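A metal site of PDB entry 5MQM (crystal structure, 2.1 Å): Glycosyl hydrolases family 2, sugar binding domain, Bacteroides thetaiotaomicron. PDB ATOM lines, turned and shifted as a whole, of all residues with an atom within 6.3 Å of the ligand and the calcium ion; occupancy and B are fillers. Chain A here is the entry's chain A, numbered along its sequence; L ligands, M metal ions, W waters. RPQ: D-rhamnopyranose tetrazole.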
ATOM      1  N   PHE A  47     -24.264  14.889  10.516  1.00  0.00           N
ATOM      2  CA  PHE A  47     -23.174  13.937  10.698  1.00  0.00           C
ATOM      3  C   PHE A  47     -22.914  13.204   9.355  1.00  0.00           C
ATOM      4  O   PHE A  47     -23.862  12.801   8.693  1.00  0.00           O
ATOM      5  CB  PHE A  47     -23.539  12.902  11.766  1.00  0.00           C
ATOM      6  CG  PHE A  47     -23.498  13.439  13.159  1.00  0.00           C
ATOM      7  CD1 PHE A  47     -22.298  13.500  13.843  1.00  0.00           C
ATOM      8  CD2 PHE A  47     -24.639  13.906  13.775  1.00  0.00           C
ATOM      9  CE1 PHE A  47     -22.232  14.025  15.123  1.00  0.00           C
ATOM     10  CE2 PHE A  47     -24.585  14.423  15.056  1.00  0.00           C
ATOM     11  CZ  PHE A  47     -23.398  14.475  15.732  1.00  0.00           C
ATOM     12  N   TYR A  49     -20.760   9.981   8.028  1.00  0.00           N
ATOM     13  CA  TYR A  49     -20.096   8.738   8.453  1.00  0.00           C
ATOM     14  C   TYR A  49     -19.458   8.026   7.250  1.00  0.00           C
ATOM     15  O   TYR A  49     -20.136   7.780   6.252  1.00  0.00           O
ATOM     16  CB  TYR A  49     -21.080   7.798   9.186  1.00  0.00           C
ATOM     17  CG  TYR A  49     -21.409   8.163  10.627  1.00  0.00           C
ATOM     18  CD1 TYR A  49     -20.939   9.368  11.213  1.00  0.00           C
ATOM     19  CD2 TYR A  49     -22.184   7.326  11.418  1.00  0.00           C
ATOM     20  CE1 TYR A  49     -21.248   9.710  12.521  1.00  0.00           C
ATOM     21  CE2 TYR A  49     -22.480   7.668  12.745  1.00  0.00           C
ATOM     22  CZ  TYR A  49     -22.000   8.857  13.280  1.00  0.00           C
ATOM     23  OH  TYR A  49     -22.263   9.223  14.590  1.00  0.00           O
ATOM     24  N   MET A  78     -16.867  11.911  10.493  1.00  0.00           N
ATOM     25  CA  MET A  78     -16.539  10.871  11.468  1.00  0.00           C
ATOM     26  C   MET A  78     -16.496   9.508  10.781  1.00  0.00           C
ATOM     27  O   MET A  78     -17.514   9.009  10.336  1.00  0.00           O
ATOM     28  CB  MET A  78     -17.576  10.859  12.578  1.00  0.00           C
ATOM     29  CG  MET A  78     -17.544  12.148  13.391  1.00  0.00           C
ATOM     30  SD  MET A  78     -18.909  12.342  14.535  1.00  0.00           S
ATOM     31  CE  MET A  78     -18.766  10.832  15.477  1.00  0.00           C
ATOM     32  N   ILE A  80     -16.298   5.465  10.737  1.00  0.00           N
ATOM     33  CA  ILE A  80     -16.778   4.434  11.609  1.00  0.00           C
ATOM     34  C   ILE A  80     -16.282   3.101  11.071  1.00  0.00           C
ATOM     35  O   ILE A  80     -16.559   2.740   9.923  1.00  0.00           O
ATOM     36  CB  ILE A  80     -18.316   4.436  11.644  1.00  0.00           C
ATOM     37  CG1 ILE A  80     -18.875   5.842  11.914  1.00  0.00           C
ATOM     38  CG2 ILE A  80     -18.810   3.450  12.677  1.00  0.00           C
ATOM     39  CD1 ILE A  80     -18.512   6.447  13.260  1.00  0.00           C
ATOM     40  N   PHE A 126     -17.393   6.776  16.750  1.00  0.00           N
ATOM     41  CA  PHE A 126     -18.307   7.801  17.299  1.00  0.00           C
ATOM     42  C   PHE A 126     -18.177   8.038  18.815  1.00  0.00           C
ATOM     43  O   PHE A 126     -18.924   8.834  19.372  1.00  0.00           O
ATOM     44  CB  PHE A 126     -19.769   7.612  16.807  1.00  0.00           C
ATOM     45  CG  PHE A 126     -20.366   6.251  17.034  1.00  0.00           C
ATOM     46  CD1 PHE A 126     -20.496   5.731  18.309  1.00  0.00           C
ATOM     47  CD2 PHE A 126     -20.900   5.520  15.959  1.00  0.00           C
ATOM     48  CE1 PHE A 126     -21.108   4.491  18.501  1.00  0.00           C
ATOM     49  CE2 PHE A 126     -21.492   4.287  16.139  1.00  0.00           C
ATOM     50  CZ  PHE A 126     -21.600   3.774  17.420  1.00  0.00           C
ATOM     51  N   ALA A 127     -17.201   7.391  19.473  1.00  0.00           N
ATOM     52  CA  ALA A 127     -16.946   7.583  20.914  1.00  0.00           C
ATOM     53  C   ALA A 127     -15.684   6.837  21.376  1.00  0.00           C
ATOM     54  O   ALA A 127     -15.480   5.699  20.939  1.00  0.00           O
ATOM     55  CB  ALA A 127     -18.138   7.098  21.744  1.00  0.00           C
ATOM     56  N   TRP A 276     -27.232   2.150  30.610  1.00  0.00           N
ATOM     57  CA  TRP A 276     -27.102   1.009  29.677  1.00  0.00           C
ATOM     58  C   TRP A 276     -25.757   0.357  29.781  1.00  0.00           C
ATOM     59  O   TRP A 276     -25.619  -0.787  29.393  1.00  0.00           O
ATOM     60  CB  TRP A 276     -27.386   1.432  28.241  1.00  0.00           C
ATOM     61  CG  TRP A 276     -26.467   2.456  27.694  1.00  0.00           C
ATOM     62  CD1 TRP A 276     -26.637   3.804  27.723  1.00  0.00           C
ATOM     63  CD2 TRP A 276     -25.221   2.204  27.054  1.00  0.00           C
ATOM     64  NE1 TRP A 276     -25.559   4.423  27.104  1.00  0.00           N
ATOM     65  CE2 TRP A 276     -24.679   3.463  26.688  1.00  0.00           C
ATOM     66  CE3 TRP A 276     -24.506   1.034  26.741  1.00  0.00           C
ATOM     67  CZ2 TRP A 276     -23.455   3.589  26.022  1.00  0.00           C
ATOM     68  CZ3 TRP A 276     -23.292   1.152  26.087  1.00  0.00           C
ATOM     69  CH2 TRP A 276     -22.776   2.426  25.735  1.00  0.00           C
ATOM     70  N   ASP A 458     -18.716  13.395  21.377  1.00  0.00           N
ATOM     71  CA  ASP A 458     -20.048  12.792  21.343  1.00  0.00           C
ATOM     72  C   ASP A 458     -20.411  12.298  22.759  1.00  0.00           C
ATOM     73  O   ASP A 458     -19.766  12.670  23.735  1.00  0.00           O
ATOM     74  CB  ASP A 458     -20.103  11.672  20.283  1.00  0.00           C
ATOM     75  CG  ASP A 458     -21.461  11.603  19.570  1.00  0.00           C
ATOM     76  OD1 ASP A 458     -21.697  12.353  18.576  1.00  0.00           O
ATOM     77  OD2 ASP A 458     -22.321  10.817  20.027  1.00  0.00           O
ATOM     78  N   SER A 459     -21.480  11.510  22.860  1.00  0.00           N
ATOM     79  CA  SER A 459     -21.963  10.954  24.134  1.00  0.00           C
ATOM     80  C   SER A 459     -21.060   9.834  24.672  1.00  0.00           C
ATOM     81  O   SER A 459     -20.627   8.962  23.919  1.00  0.00           O
ATOM     82  CB  SER A 459     -23.424  10.506  23.998  1.00  0.00           C
ATOM     83  OG  SER A 459     -23.679   9.941  22.726  1.00  0.00           O
ATOM     84  N   GLU A 461     -19.369   6.642  26.104  1.00  0.00           N
ATOM     85  CA  GLU A 461     -19.611   5.193  26.024  1.00  0.00           C
ATOM     86  C   GLU A 461     -18.419   4.369  26.520  1.00  0.00           C
ATOM     87  O   GLU A 461     -18.282   3.233  26.112  1.00  0.00           O
ATOM     88  CB  GLU A 461     -19.904   4.774  24.579  1.00  0.00           C
ATOM     89  CG  GLU A 461     -20.946   5.611  23.881  1.00  0.00           C
ATOM     90  CD  GLU A 461     -21.468   4.994  22.586  1.00  0.00           C
ATOM     91  OE1 GLU A 461     -20.815   4.089  21.997  1.00  0.00           O
ATOM     92  OE2 GLU A 461     -22.567   5.454  22.177  1.00  0.00           O
ATOM     93  N   GLU A 538     -21.807  16.417  23.648  1.00  0.00           N
ATOM     94  CA  GLU A 538     -23.014  15.681  24.047  1.00  0.00           C
ATOM     95  C   GLU A 538     -22.857  15.210  25.504  1.00  0.00           C
ATOM     96  O   GLU A 538     -21.999  15.712  26.213  1.00  0.00           O
ATOM     97  CB  GLU A 538     -23.269  14.518  23.077  1.00  0.00           C
ATOM     98  CG  GLU A 538     -23.687  14.964  21.687  1.00  0.00           C
ATOM     99  CD  GLU A 538     -24.232  13.824  20.826  1.00  0.00           C
ATOM    100  OE1 GLU A 538     -24.223  12.667  21.294  1.00  0.00           O
ATOM    101  OE2 GLU A 538     -24.639  14.092  19.675  1.00  0.00           O
ATOM    102  N   GLU A 561     -29.679  14.809  22.016  1.00  0.00           N
ATOM    103  CA  GLU A 561     -29.955  13.789  21.021  1.00  0.00           C
ATOM    104  C   GLU A 561     -31.425  13.349  21.129  1.00  0.00           C
ATOM    105  O   GLU A 561     -31.979  13.229  22.239  1.00  0.00           O
ATOM    106  CB  GLU A 561     -28.897  12.668  21.175  1.00  0.00           C
ATOM    107  CG  GLU A 561     -29.346  11.239  21.203  1.00  0.00           C
ATOM    108  CD  GLU A 561     -28.178  10.265  21.386  1.00  0.00           C
ATOM    109  OE1 GLU A 561     -27.099  10.675  21.858  1.00  0.00           O
ATOM    110  OE2 GLU A 561     -28.359   9.063  21.054  1.00  0.00           O
ATOM    111  N   TRP A 563     -34.160  10.467  19.140  1.00  0.00           N
ATOM    112  CA  TRP A 563     -34.309   9.369  18.193  1.00  0.00           C
ATOM    113  C   TRP A 563     -35.696   9.321  17.553  1.00  0.00           C
ATOM    114  O   TRP A 563     -36.700   9.803  18.110  1.00  0.00           O
ATOM    115  CB  TRP A 563     -34.013   8.051  18.883  1.00  0.00           C
ATOM    116  CG  TRP A 563     -32.585   7.853  19.287  1.00  0.00           C
ATOM    117  CD1 TRP A 563     -31.816   8.661  20.104  1.00  0.00           C
ATOM    118  CD2 TRP A 563     -31.751   6.744  18.945  1.00  0.00           C
ATOM    119  NE1 TRP A 563     -30.576   8.150  20.245  1.00  0.00           N
ATOM    120  CE2 TRP A 563     -30.502   6.955  19.575  1.00  0.00           C
ATOM    121  CE3 TRP A 563     -31.948   5.586  18.189  1.00  0.00           C
ATOM    122  CZ2 TRP A 563     -29.441   6.049  19.466  1.00  0.00           C
ATOM    123  CZ3 TRP A 563     -30.888   4.679  18.070  1.00  0.00           C
ATOM    124  CH2 TRP A 563     -29.655   4.914  18.711  1.00  0.00           C
ATOM    125  N   HIS A 569     -33.907   3.174  22.690  1.00  0.00           N
ATOM    126  CA  HIS A 569     -32.604   3.861  22.552  1.00  0.00           C
ATOM    127  C   HIS A 569     -32.677   5.418  22.588  1.00  0.00           C
ATOM    128  O   HIS A 569     -31.618   6.119  22.523  1.00  0.00           O
ATOM    129  CB  HIS A 569     -31.976   3.487  21.223  1.00  0.00           C
ATOM    130  CG  HIS A 569     -31.412   2.098  21.214  1.00  0.00           C
ATOM    131  ND1 HIS A 569     -32.209   0.974  21.325  1.00  0.00           N
ATOM    132  CD2 HIS A 569     -30.141   1.656  21.105  1.00  0.00           C
ATOM    133  CE1 HIS A 569     -31.440  -0.103  21.314  1.00  0.00           C
ATOM    134  NE2 HIS A 569     -30.187   0.288  21.177  1.00  0.00           N
ATOM    135  N   LYS A 571     -33.056   9.254  24.060  1.00  0.00           N
ATOM    136  CA  LYS A 571     -32.441   9.856  25.222  1.00  0.00           C
ATOM    137  C   LYS A 571     -33.037  11.213  25.580  1.00  0.00           C
ATOM    138  O   LYS A 571     -32.379  12.238  25.472  1.00  0.00           O
ATOM    139  CB  LYS A 571     -30.923   9.926  25.014  1.00  0.00           C
ATOM    140  CG  LYS A 571     -30.296   8.547  24.845  1.00  0.00           C
ATOM    141  CD  LYS A 571     -28.780   8.609  24.951  1.00  0.00           C
ATOM    142  CE  LYS A 571     -28.091   7.350  24.465  1.00  0.00           C
ATOM    143  NZ  LYS A 571     -27.652   7.455  23.037  1.00  0.00           N
ATOM    144  N   ASP A 574     -30.981  13.029  28.054  1.00  0.00           N
ATOM    145  CA  ASP A 574     -29.776  13.659  27.458  1.00  0.00           C
ATOM    146  C   ASP A 574     -30.152  15.037  26.866  1.00  0.00           C
ATOM    147  O   ASP A 574     -29.370  15.994  26.937  1.00  0.00           O
ATOM    148  CB  ASP A 574     -29.156  12.852  26.312  1.00  0.00           C
ATOM    149  CG  ASP A 574     -28.328  11.657  26.764  1.00  0.00           C
ATOM    150  OD1 ASP A 574     -28.569  11.040  27.856  1.00  0.00           O
ATOM    151  OD2 ASP A 574     -27.417  11.313  25.941  1.00  0.00           O
ATOM    152  N   GLU A 593     -28.326  16.110  17.831  1.00  0.00           N
ATOM    153  CA  GLU A 593     -28.255  14.960  16.918  1.00  0.00           C
ATOM    154  C   GLU A 593     -29.667  14.443  16.779  1.00  0.00           C
ATOM    155  O   GLU A 593     -30.239  13.951  17.748  1.00  0.00           O
ATOM    156  CB  GLU A 593     -27.329  13.922  17.530  1.00  0.00           C
ATOM    157  CG  GLU A 593     -27.292  12.562  16.873  1.00  0.00           C
ATOM    158  CD  GLU A 593     -26.732  11.515  17.838  1.00  0.00           C
ATOM    159  OE1 GLU A 593     -25.738  11.844  18.558  1.00  0.00           O
ATOM    160  OE2 GLU A 593     -27.304  10.390  17.869  1.00  0.00           O
ATOM    161  N   THR A 596     -31.959   9.849  14.813  1.00  0.00           N
ATOM    162  CA  THR A 596     -31.255   8.570  14.962  1.00  0.00           C
ATOM    163  C   THR A 596     -32.308   7.479  15.106  1.00  0.00           C
ATOM    164  O   THR A 596     -33.230   7.598  15.901  1.00  0.00           O
ATOM    165  CB  THR A 596     -30.366   8.617  16.194  1.00  0.00           C
ATOM    166  OG1 THR A 596     -29.656   9.856  16.210  1.00  0.00           O
ATOM    167  CG2 THR A 596     -29.399   7.471  16.220  1.00  0.00           C
ATOM    168  N   HIS A 627     -28.914  12.947  11.861  1.00  0.00           N
ATOM    169  CA  HIS A 627     -28.261  11.657  12.017  1.00  0.00           C
ATOM    170  C   HIS A 627     -28.990  10.693  11.080  1.00  0.00           C
ATOM    171  O   HIS A 627     -30.114  10.353  11.369  1.00  0.00           O
ATOM    172  CB  HIS A 627     -28.339  11.159  13.435  1.00  0.00           C
ATOM    173  CG  HIS A 627     -27.577   9.885  13.626  1.00  0.00           C
ATOM    174  ND1 HIS A 627     -27.969   8.700  13.059  1.00  0.00           N
ATOM    175  CD2 HIS A 627     -26.377   9.664  14.203  1.00  0.00           C
ATOM    176  CE1 HIS A 627     -27.078   7.776  13.327  1.00  0.00           C
ATOM    177  NE2 HIS A 627     -26.102   8.329  14.018  1.00  0.00           N
ATOM    178  N   VAL A 628     -28.409  10.240   9.973  1.00  0.00           N
ATOM    179  CA  VAL A 628     -27.018  10.400   9.607  1.00  0.00           C
ATOM    180  C   VAL A 628     -26.854  10.391   8.090  1.00  0.00           C
ATOM    181  O   VAL A 628     -27.583   9.695   7.363  1.00  0.00           O
ATOM    182  CB  VAL A 628     -26.176   9.267  10.255  1.00  0.00           C
ATOM    183  CG1 VAL A 628     -26.652   7.883   9.851  1.00  0.00           C
ATOM    184  CG2 VAL A 628     -24.691   9.457   9.946  1.00  0.00           C
ATOM    185  N   LEU A 643     -25.038   2.884   7.884  1.00  0.00           N
ATOM    186  CA  LEU A 643     -24.515   2.456   9.188  1.00  0.00           C
ATOM    187  C   LEU A 643     -25.210   1.154   9.617  1.00  0.00           C
ATOM    188  O   LEU A 643     -25.956   1.119  10.628  1.00  0.00           O
ATOM    189  CB  LEU A 643     -24.799   3.568  10.244  1.00  0.00           C
ATOM    190  CG  LEU A 643     -24.265   3.430  11.663  1.00  0.00           C
ATOM    191  CD1 LEU A 643     -22.743   3.278  11.618  1.00  0.00           C
ATOM    192  CD2 LEU A 643     -24.672   4.620  12.530  1.00  0.00           C
ATOM    193  N   ILE A 646     -28.939   1.466  10.578  1.00  0.00           N
ATOM    194  CA  ILE A 646     -29.271   2.432  11.607  1.00  0.00           C
ATOM    195  C   ILE A 646     -29.512   3.734  10.809  1.00  0.00           C
ATOM    196  O   ILE A 646     -28.624   4.213  10.091  1.00  0.00           O
ATOM    197  CB  ILE A 646     -28.122   2.596  12.637  1.00  0.00           C
ATOM    198  CG1 ILE A 646     -27.926   1.313  13.460  1.00  0.00           C
ATOM    199  CG2 ILE A 646     -28.389   3.760  13.596  1.00  0.00           C
ATOM    200  CD1 ILE A 646     -26.682   1.299  14.344  1.00  0.00           C
ATOM    201  N   GLY A 647     -30.715   4.268  10.935  1.00  0.00           N
ATOM    202  CA  GLY A 647     -31.071   5.516  10.266  1.00  0.00           C
ATOM    203  C   GLY A 647     -30.790   6.738  11.119  1.00  0.00           C
ATOM    204  O   GLY A 647     -30.095   6.639  12.141  1.00  0.00           O
HETATM  205  O3  RPQ L   1     -24.114   9.314  18.259  1.00  0.00           O
HETATM  206  C3  RPQ L   1     -23.722   7.950  18.070  1.00  0.00           C
HETATM  207  C4  RPQ L   1     -24.648   7.303  17.014  1.00  0.00           C
HETATM  208  O4  RPQ L   1     -24.115   7.573  15.697  1.00  0.00           O
HETATM  209  C2  RPQ L   1     -23.623   7.258  19.444  1.00  0.00           C
HETATM  210  O2  RPQ L   1     -23.729   8.183  20.535  1.00  0.00           O
HETATM  211  C1  RPQ L   1     -24.689   6.251  19.615  1.00  0.00           C
HETATM  212  N20 RPQ L   1     -25.288   5.837  20.756  1.00  0.00           N
HETATM  213  N2  RPQ L   1     -26.207   4.886  20.320  1.00  0.00           N
HETATM  214  N1  RPQ L   1     -26.210   4.689  18.935  1.00  0.00           N
HETATM  215  N5  RPQ L   1     -25.202   5.612  18.584  1.00  0.00           N
HETATM  216  C5  RPQ L   1     -24.841   5.781  17.173  1.00  0.00           C
HETATM  217  C6  RPQ L   1     -25.906   5.176  16.255  1.00  0.00           C
HETATM  218 CA    CA M   1     -24.742  10.485  20.388  1.00  0.00          CA
HETATM  219  O   HOH W   1     -24.146   7.177  23.659  1.00  0.00           O
HETATM  220  O   HOH W   2     -21.216   8.294  21.434  1.00  0.00           O
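An oxygen (O4) of the ligand sits at hydrogen-bond distance from the side-chain hydroxyl (OH) of Tyr 49 (2.7 Å).
NE2 of His 627 is in hydrogen-bond range of O4 of the ligand (2.7 Å).
The side-chain carboxylate (OE2) of Glu 461 sits close to an oxygen (O2) of the ligand, 3.4 Å away.
A ring nitrogen (ND1) of His 627 lies within hydrogen-bond range of the backbone carbonyl oxygen (O) of Gly 647 (3.1 Å).
The side-chain carboxylate (OE2) of Glu 593 lies within hydrogen-bond range of the side-chain hydroxyl (OG1) of Thr 596, 2.9 Å away.
The backbone carbonyl oxygen (O) of His 569 sits at hydrogen-bond distance from the indole nitrogen (NE1) of Trp 563 (3.2 Å).
OE2 of Glu 561 lies within salt-bridge range of NZ of Lys 571 (2.6 Å).
OE2 of Glu 561 is in hydrogen-bond range of NE1 of Trp 563 (2.5 Å).
Phe 126 touches the ligand (CD1 to C2, 3.7 Å).
CH2 of Trp 563 touches N1 of the ligand, 3.5 Å away.
NZ of Lys 571 touches N20 of the ligand (3.7 Å).
CD2 of Leu 643 touches C6 of the ligand, 3.96 Å away.
CG2 of Ile 646 touches C6 of the ligand (3.9 Å).
Hydrophobic or aromatic side chains within 4 Å of the ligand: Tyr 49, Phe 126, Trp 563, His 627, Leu 643 and Ile 646.
Of the 23 residues printed, 5 come within 4 Å of the calcium ion.
Along chain A the residues within 4 Å of the calcium ion span positions 458 to 593.
The calcium ion is bound by the side-chain carboxylate of Glu 538, the side-chain carboxylate of Asp 458, the side-chain carboxylate of Glu 593, an oxygen (O3) of the ligand, an oxygen (O2) of the ligand, the side-chain hydroxyl of Ser 459 and the side-chain carboxylate of Glu 561.
The calcium ion has seven donor atoms within binding distance.
Water W1 bridges OE2 of Glu 461 and N20 of the ligand.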
